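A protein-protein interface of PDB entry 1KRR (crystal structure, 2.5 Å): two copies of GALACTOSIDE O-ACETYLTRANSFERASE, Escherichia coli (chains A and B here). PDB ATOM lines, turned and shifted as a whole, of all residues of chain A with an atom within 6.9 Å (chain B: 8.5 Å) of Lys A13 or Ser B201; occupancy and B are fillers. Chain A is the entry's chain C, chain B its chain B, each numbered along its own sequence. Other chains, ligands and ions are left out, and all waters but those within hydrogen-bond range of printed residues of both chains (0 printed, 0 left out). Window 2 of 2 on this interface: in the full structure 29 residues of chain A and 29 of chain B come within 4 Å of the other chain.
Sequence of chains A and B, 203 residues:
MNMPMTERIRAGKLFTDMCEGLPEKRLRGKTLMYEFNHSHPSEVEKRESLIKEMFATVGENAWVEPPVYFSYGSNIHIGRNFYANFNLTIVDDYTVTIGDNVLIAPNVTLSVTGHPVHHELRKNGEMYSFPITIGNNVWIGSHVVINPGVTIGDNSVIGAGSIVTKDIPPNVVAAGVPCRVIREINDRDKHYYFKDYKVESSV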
ATOM      1  N   ASN A   2       1.619  -3.871  28.532  1.00  0.00           N
ATOM      2  CA  ASN A   2       2.032  -3.599  27.118  1.00  0.00           C
ATOM      3  C   ASN A   2       0.783  -3.293  26.241  1.00  0.00           C
ATOM      4  O   ASN A   2      -0.205  -2.704  26.728  1.00  0.00           O
ATOM      5  CB  ASN A   2       2.813  -4.818  26.550  1.00  0.00           C
ATOM      6  CG  ASN A   2       4.032  -5.235  27.432  1.00  0.00           C
ATOM      7  OD1 ASN A   2       4.974  -4.451  27.649  1.00  0.00           O
ATOM      8  ND2 ASN A   2       4.012  -6.486  27.920  1.00  0.00           N
ATOM      9  N   MET A   3       0.853  -3.680  24.958  1.00  0.00           N
ATOM     10  CA  MET A   3      -0.224  -3.487  23.964  1.00  0.00           C
ATOM     11  C   MET A   3      -0.071  -4.546  22.817  1.00  0.00           C
ATOM     12  O   MET A   3       0.959  -5.226  22.743  1.00  0.00           O
ATOM     13  CB  MET A   3      -0.187  -2.031  23.405  1.00  0.00           C
ATOM     14  CG  MET A   3       1.085  -1.562  22.668  1.00  0.00           C
ATOM     15  SD  MET A   3       0.675  -0.465  21.276  1.00  0.00           S
ATOM     16  CE  MET A   3       2.181   0.577  21.143  1.00  0.00           C
ATOM     17  N   MET A   5       0.807  -6.958  19.750  1.00  0.00           N
ATOM     18  CA  MET A   5       2.128  -7.121  19.133  1.00  0.00           C
ATOM     19  C   MET A   5       2.331  -6.375  17.809  1.00  0.00           C
ATOM     20  O   MET A   5       3.375  -5.754  17.606  1.00  0.00           O
ATOM     21  CB  MET A   5       2.466  -8.610  18.957  1.00  0.00           C
ATOM     22  CG  MET A   5       3.051  -9.301  20.208  1.00  0.00           C
ATOM     23  SD  MET A   5       4.008  -8.238  21.325  1.00  0.00           S
ATOM     24  CE  MET A   5       3.631  -8.779  22.900  1.00  0.00           C
ATOM     25  N   GLU A   7       1.085  -3.689  16.899  1.00  0.00           N
ATOM     26  CA  GLU A   7       1.203  -2.274  17.214  1.00  0.00           C
ATOM     27  C   GLU A   7       2.607  -1.954  17.704  1.00  0.00           C
ATOM     28  O   GLU A   7       3.226  -1.015  17.231  1.00  0.00           O
ATOM     29  CB  GLU A   7       0.220  -1.887  18.309  1.00  0.00           C
ATOM     30  CG  GLU A   7      -1.209  -2.239  18.003  1.00  0.00           C
ATOM     31  CD  GLU A   7      -2.175  -1.404  18.816  1.00  0.00           C
ATOM     32  OE1 GLU A   7      -1.747  -0.825  19.850  1.00  0.00           O
ATOM     33  OE2 GLU A   7      -3.361  -1.320  18.416  1.00  0.00           O
ATOM     34  N   ARG A   8       3.095  -2.723  18.672  1.00  0.00           N
ATOM     35  CA  ARG A   8       4.432  -2.498  19.203  1.00  0.00           C
ATOM     36  C   ARG A   8       5.375  -2.353  18.026  1.00  0.00           C
ATOM     37  O   ARG A   8       6.255  -1.494  18.019  1.00  0.00           O
ATOM     38  CB  ARG A   8       4.879  -3.677  20.066  1.00  0.00           C
ATOM     39  CG  ARG A   8       3.796  -4.252  20.973  1.00  0.00           C
ATOM     40  CD  ARG A   8       3.902  -3.717  22.397  1.00  0.00           C
ATOM     41  NE  ARG A   8       4.824  -4.497  23.209  1.00  0.00           N
ATOM     42  CZ  ARG A   8       5.654  -3.976  24.107  1.00  0.00           C
ATOM     43  NH1 ARG A   8       5.680  -2.664  24.315  1.00  0.00           N
ATOM     44  NH2 ARG A   8       6.469  -4.770  24.795  1.00  0.00           N
ATOM     45  N   ILE A   9       5.177  -3.194  17.018  1.00  0.00           N
ATOM     46  CA  ILE A   9       6.011  -3.157  15.833  1.00  0.00           C
ATOM     47  C   ILE A   9       5.992  -1.751  15.270  1.00  0.00           C
ATOM     48  O   ILE A   9       6.999  -1.052  15.293  1.00  0.00           O
ATOM     49  CB  ILE A   9       5.512  -4.149  14.771  1.00  0.00           C
ATOM     50  CG1 ILE A   9       5.479  -5.558  15.358  1.00  0.00           C
ATOM     51  CG2 ILE A   9       6.437  -4.138  13.577  1.00  0.00           C
ATOM     52  CD1 ILE A   9       5.158  -6.630  14.345  1.00  0.00           C
ATOM     53  N   ARG A  10       4.834  -1.335  14.783  1.00  0.00           N
ATOM     54  CA  ARG A  10       4.674  -0.003  14.221  1.00  0.00           C
ATOM     55  C   ARG A  10       5.163   1.123  15.140  1.00  0.00           C
ATOM     56  O   ARG A  10       5.558   2.175  14.662  1.00  0.00           O
ATOM     57  CB  ARG A  10       3.205   0.235  13.879  1.00  0.00           C
ATOM     58  CG  ARG A  10       2.829  -0.226  12.482  1.00  0.00           C
ATOM     59  CD  ARG A  10       1.373   0.054  12.180  1.00  0.00           C
ATOM     60  NE  ARG A  10       0.596  -1.174  12.164  1.00  0.00           N
ATOM     61  CZ  ARG A  10      -0.306  -1.485  13.093  1.00  0.00           C
ATOM     62  NH1 ARG A  10      -0.537  -0.652  14.103  1.00  0.00           N
ATOM     63  NH2 ARG A  10      -0.972  -2.628  13.016  1.00  0.00           N
ATOM     64  N   ALA A  11       5.135   0.899  16.450  1.00  0.00           N
ATOM     65  CA  ALA A  11       5.559   1.912  17.419  1.00  0.00           C
ATOM     66  C   ALA A  11       7.026   1.815  17.815  1.00  0.00           C
ATOM     67  O   ALA A  11       7.494   2.572  18.676  1.00  0.00           O
ATOM     68  CB  ALA A  11       4.693   1.832  18.669  1.00  0.00           C
ATOM     69  N   GLY A  12       7.750   0.885  17.202  1.00  0.00           N
ATOM     70  CA  GLY A  12       9.149   0.740  17.538  1.00  0.00           C
ATOM     71  C   GLY A  12       9.317   0.257  18.962  1.00  0.00           C
ATOM     72  O   GLY A  12      10.234   0.670  19.650  1.00  0.00           O
ATOM     73  N   LYS A  13       8.432  -0.629  19.403  1.00  0.00           N
ATOM     74  CA  LYS A  13       8.488  -1.181  20.757  1.00  0.00           C
ATOM     75  C   LYS A  13       8.926  -2.635  20.686  1.00  0.00           C
ATOM     76  O   LYS A  13       8.734  -3.279  19.656  1.00  0.00           O
ATOM     77  CB  LYS A  13       7.111  -1.127  21.413  1.00  0.00           C
ATOM     78  CG  LYS A  13       6.748   0.229  21.947  1.00  0.00           C
ATOM     79  CD  LYS A  13       5.315   0.560  21.636  1.00  0.00           C
ATOM     80  CE  LYS A  13       4.699   1.304  22.795  1.00  0.00           C
ATOM     81  NZ  LYS A  13       4.387   0.353  23.892  1.00  0.00           N
ATOM     82  N   LEU A  14       9.500  -3.138  21.781  1.00  0.00           N
ATOM     83  CA  LEU A  14       9.957  -4.530  21.871  1.00  0.00           C
ATOM     84  C   LEU A  14       8.774  -5.489  21.697  1.00  0.00           C
ATOM     85  O   LEU A  14       7.692  -5.262  22.244  1.00  0.00           O
ATOM     86  CB  LEU A  14      10.639  -4.785  23.220  1.00  0.00           C
ATOM     87  CG  LEU A  14      12.001  -4.100  23.342  1.00  0.00           C
ATOM     88  CD1 LEU A  14      12.463  -4.168  24.765  1.00  0.00           C
ATOM     89  CD2 LEU A  14      13.014  -4.754  22.420  1.00  0.00           C
ATOM     90  N   PHE A  15       8.988  -6.556  20.932  1.00  0.00           N
ATOM     91  CA  PHE A  15       7.942  -7.522  20.669  1.00  0.00           C
ATOM     92  C   PHE A  15       8.518  -8.894  20.356  1.00  0.00           C
ATOM     93  O   PHE A  15       9.714  -9.054  20.087  1.00  0.00           O
ATOM     94  CB  PHE A  15       7.113  -7.072  19.462  1.00  0.00           C
ATOM     95  CG  PHE A  15       7.863  -7.152  18.145  1.00  0.00           C
ATOM     96  CD1 PHE A  15       8.803  -6.171  17.799  1.00  0.00           C
ATOM     97  CD2 PHE A  15       7.635  -8.209  17.254  1.00  0.00           C
ATOM     98  CE1 PHE A  15       9.498  -6.243  16.591  1.00  0.00           C
ATOM     99  CE2 PHE A  15       8.329  -8.286  16.042  1.00  0.00           C
ATOM    100  CZ  PHE A  15       9.259  -7.302  15.712  1.00  0.00           C
ATOM    101  N   THR A  16       7.623  -9.873  20.419  1.00  0.00           N
ATOM    102  CA  THR A  16       7.907 -11.254  20.084  1.00  0.00           C
ATOM    103  C   THR A  16       6.909 -11.570  18.968  1.00  0.00           C
ATOM    104  O   THR A  16       5.860 -10.931  18.866  1.00  0.00           O
ATOM    105  CB  THR A  16       7.704 -12.177  21.288  1.00  0.00           C
ATOM    106  OG1 THR A  16       6.370 -12.044  21.767  1.00  0.00           O
ATOM    107  CG2 THR A  16       8.650 -11.824  22.431  1.00  0.00           C
ATOM    108  N   MET A 127      12.459  -8.557  20.142  1.00  0.00           N
ATOM    109  CA  MET A 127      13.136  -7.722  19.193  1.00  0.00           C
ATOM    110  C   MET A 127      12.394  -6.444  18.893  1.00  0.00           C
ATOM    111  O   MET A 127      11.262  -6.269  19.327  1.00  0.00           O
ATOM    112  CB  MET A 127      13.341  -8.505  17.890  1.00  0.00           C
ATOM    113  CG  MET A 127      12.046  -8.941  17.202  1.00  0.00           C
ATOM    114  SD  MET A 127      11.873 -10.731  17.133  1.00  0.00           S
ATOM    115  CE  MET A 127      10.372 -10.886  16.177  1.00  0.00           C
ATOM    116  N   TYR A 128      13.042  -5.553  18.141  1.00  0.00           N
ATOM    117  CA  TYR A 128      12.433  -4.294  17.737  1.00  0.00           C
ATOM    118  C   TYR A 128      12.665  -4.197  16.237  1.00  0.00           C
ATOM    119  O   TYR A 128      13.557  -4.858  15.700  1.00  0.00           O
ATOM    120  CB  TYR A 128      13.065  -3.094  18.471  1.00  0.00           C
ATOM    121  CG  TYR A 128      14.565  -3.070  18.364  1.00  0.00           C
ATOM    122  CD1 TYR A 128      15.176  -2.734  17.164  1.00  0.00           C
ATOM    123  CD2 TYR A 128      15.372  -3.423  19.445  1.00  0.00           C
ATOM    124  CE1 TYR A 128      16.539  -2.753  17.028  1.00  0.00           C
ATOM    125  CE2 TYR A 128      16.736  -3.443  19.321  1.00  0.00           C
ATOM    126  CZ  TYR A 128      17.321  -3.107  18.103  1.00  0.00           C
ATOM    127  OH  TYR A 128      18.693  -3.132  17.964  1.00  0.00           O
ATOM    128  N   SER A 129      11.861  -3.387  15.557  1.00  0.00           N
ATOM    129  CA  SER A 129      12.000  -3.239  14.121  1.00  0.00           C
ATOM    130  C   SER A 129      11.798  -1.808  13.686  1.00  0.00           C
ATOM    131  O   SER A 129      10.804  -1.189  14.037  1.00  0.00           O
ATOM    132  CB  SER A 129      10.983  -4.126  13.408  1.00  0.00           C
ATOM    133  OG  SER A 129      11.507  -5.422  13.187  1.00  0.00           O
ATOM    134  N   PHE A 130      12.740  -1.283  12.914  1.00  0.00           N
ATOM    135  CA  PHE A 130      12.631   0.076  12.417  1.00  0.00           C
ATOM    136  C   PHE A 130      12.829   0.000  10.924  1.00  0.00           C
ATOM    137  O   PHE A 130      13.824  -0.533  10.435  1.00  0.00           O
ATOM    138  CB  PHE A 130      13.651   0.996  13.107  1.00  0.00           C
ATOM    139  CG  PHE A 130      13.367   1.198  14.558  1.00  0.00           C
ATOM    140  CD1 PHE A 130      12.326   2.036  14.936  1.00  0.00           C
ATOM    141  CD2 PHE A 130      14.121   0.563  15.550  1.00  0.00           C
ATOM    142  CE1 PHE A 130      12.031   2.244  16.270  1.00  0.00           C
ATOM    143  CE2 PHE A 130      13.839   0.762  16.895  1.00  0.00           C
ATOM    144  CZ  PHE A 130      12.785   1.610  17.260  1.00  0.00           C
ATOM    145  N   HIS B 191      17.246   0.152  30.114  1.00  0.00           N
ATOM    146  CA  HIS B 191      16.286   1.203  29.777  1.00  0.00           C
ATOM    147  C   HIS B 191      16.260   1.539  28.301  1.00  0.00           C
ATOM    148  O   HIS B 191      15.192   1.670  27.708  1.00  0.00           O
ATOM    149  CB  HIS B 191      16.619   2.454  30.566  1.00  0.00           C
ATOM    150  CG  HIS B 191      16.684   2.218  32.036  1.00  0.00           C
ATOM    151  ND1 HIS B 191      17.872   1.994  32.700  1.00  0.00           N
ATOM    152  CD2 HIS B 191      15.705   2.129  32.968  1.00  0.00           C
ATOM    153  CE1 HIS B 191      17.620   1.777  33.981  1.00  0.00           C
ATOM    154  NE2 HIS B 191      16.313   1.853  34.169  1.00  0.00           N
ATOM    155  N   TYR B 193      16.962   0.356  24.624  1.00  0.00           N
ATOM    156  CA  TYR B 193      17.140  -0.883  23.882  1.00  0.00           C
ATOM    157  C   TYR B 193      17.577  -0.632  22.454  1.00  0.00           C
ATOM    158  O   TYR B 193      17.931  -1.568  21.740  1.00  0.00           O
ATOM    159  CB  TYR B 193      15.858  -1.720  23.897  1.00  0.00           C
ATOM    160  CG  TYR B 193      14.683  -1.041  23.251  1.00  0.00           C
ATOM    161  CD1 TYR B 193      14.559  -0.983  21.863  1.00  0.00           C
ATOM    162  CD2 TYR B 193      13.696  -0.445  24.029  1.00  0.00           C
ATOM    163  CE1 TYR B 193      13.481  -0.346  21.275  1.00  0.00           C
ATOM    164  CE2 TYR B 193      12.617   0.193  23.454  1.00  0.00           C
ATOM    165  CZ  TYR B 193      12.514   0.238  22.082  1.00  0.00           C
ATOM    166  OH  TYR B 193      11.420   0.855  21.539  1.00  0.00           O
ATOM    167  N   TYR B 197      15.720   5.168  22.042  1.00  0.00           N
ATOM    168  CA  TYR B 197      14.415   4.626  22.387  1.00  0.00           C
ATOM    169  C   TYR B 197      14.446   4.039  23.786  1.00  0.00           C
ATOM    170  O   TYR B 197      15.181   3.093  24.054  1.00  0.00           O
ATOM    171  CB  TYR B 197      14.011   3.562  21.366  1.00  0.00           C
ATOM    172  CG  TYR B 197      13.468   4.141  20.077  1.00  0.00           C
ATOM    173  CD1 TYR B 197      14.322   4.579  19.063  1.00  0.00           C
ATOM    174  CD2 TYR B 197      12.097   4.261  19.873  1.00  0.00           C
ATOM    175  CE1 TYR B 197      13.815   5.127  17.868  1.00  0.00           C
ATOM    176  CE2 TYR B 197      11.581   4.804  18.692  1.00  0.00           C
ATOM    177  CZ  TYR B 197      12.440   5.234  17.694  1.00  0.00           C
ATOM    178  OH  TYR B 197      11.905   5.745  16.525  1.00  0.00           O
ATOM    179  N   LYS B 198      13.646   4.618  24.677  1.00  0.00           N
ATOM    180  CA  LYS B 198      13.558   4.176  26.068  1.00  0.00           C
ATOM    181  C   LYS B 198      12.532   3.058  26.219  1.00  0.00           C
ATOM    182  O   LYS B 198      11.471   3.084  25.589  1.00  0.00           O
ATOM    183  CB  LYS B 198      13.184   5.356  26.973  1.00  0.00           C
ATOM    184  N   VAL B 199      12.853   2.081  27.063  1.00  0.00           N
ATOM    185  CA  VAL B 199      11.969   0.948  27.296  1.00  0.00           C
ATOM    186  C   VAL B 199      10.585   1.374  27.727  1.00  0.00           C
ATOM    187  O   VAL B 199       9.618   0.647  27.501  1.00  0.00           O
ATOM    188  CB  VAL B 199      12.519   0.011  28.385  1.00  0.00           C
ATOM    189  CG1 VAL B 199      11.430  -0.940  28.860  1.00  0.00           C
ATOM    190  CG2 VAL B 199      13.679  -0.782  27.842  1.00  0.00           C
ATOM    191  N   GLU B 200      10.479   2.540  28.359  1.00  0.00           N
ATOM    192  CA  GLU B 200       9.174   3.000  28.807  1.00  0.00           C
ATOM    193  C   GLU B 200       8.573   4.144  27.991  1.00  0.00           C
ATOM    194  O   GLU B 200       8.781   5.326  28.297  1.00  0.00           O
ATOM    195  CB  GLU B 200       9.219   3.390  30.285  1.00  0.00           C
ATOM    196  CG  GLU B 200       7.958   2.985  31.041  1.00  0.00           C
ATOM    197  CD  GLU B 200       8.219   1.893  32.059  1.00  0.00           C
ATOM    198  OE1 GLU B 200       8.773   0.830  31.674  1.00  0.00           O
ATOM    199  OE2 GLU B 200       7.866   2.101  33.248  1.00  0.00           O
ATOM    200  N   SER B 201       7.840   3.762  26.942  1.00  0.00           N
ATOM    201  CA  SER B 201       7.136   4.691  26.060  1.00  0.00           C
ATOM    202  C   SER B 201       5.672   4.448  26.415  1.00  0.00           C
ATOM    203  O   SER B 201       5.331   3.340  26.849  1.00  0.00           O
ATOM    204  CB  SER B 201       7.382   4.338  24.586  1.00  0.00           C
ATOM    205  OG  SER B 201       6.392   3.446  24.089  1.00  0.00           O
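Of the printed residues of chain B, Lys A13 touches Tyr B193 and Ser B201. Of chain A, only Lys A13 comes within 4 Å of Ser B201. Of chain B, only Tyr B193 comes within 4 Å of Gly A12. Of the printed residues of chain A, Tyr B197 touches Phe A130 (3.3 Å). Printed residues of chain B within 4 Å of Tyr A128: Tyr B193 (3.3 Å). Of the printed residues of chain B, Leu A14 touches Tyr B193 (3.99 Å). Of the printed residues of chain B, Phe A130 touches Tyr B197 (3.3 Å). Of the printed residues of chain A, Tyr B193 touches Gly A12 (2.2 Å), Lys A13 (3.7 Å), Leu A14 (3.99 Å) and Tyr A128 (3.3 Å). Ile A9 touches none of the printed residues of chain B. Glu B200 touches none of the printed residues of chain A. The nearest residue of chain B that does not touch Lys A13 is Tyr B197 (6.1 Å). The nearest printed residue of chain B that does not touch Phe A130 is Tyr B193 (4.5 Å).
No position is printed for both chains. Of the 6 pairs that touch across the chains among the printed residues, none has its exchanged pair printed and touching as well.
The side-chain hydroxyl (OH) of Tyr B193 lies close to the backbone carbonyl oxygen (O) of Gly A12 (2.2 Å).
Printed residues of chain A that touch a printed residue of chain B: Gly A12, Lys A13, Leu A14, Tyr A128 and Phe A130. Hydrophobic or aromatic side chains of chain A within 4 Å of the printed part of chain B: Leu A14, Tyr A128 and Phe A130. Of the 7 printed residues of chain B, 3 touch a printed residue of chain A. Among the printed residues, 6 pairs touch across the chains.
The backbone NH (N) of Lys A13 lies within hydrogen-bond range of the backbone carbonyl oxygen (O) of Arg A8 (2.7 Å). NH2 of Arg A8 is in hydrogen-bond range of O of Leu A14 (2.9 Å).
Among the printed residues, merely in contact across the chains: Lys A13 with Tyr B193, Lys A13 with Ser B201, Leu A14 with Tyr B193, Tyr A128 with Tyr B193 and Phe A130 with Tyr B197.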
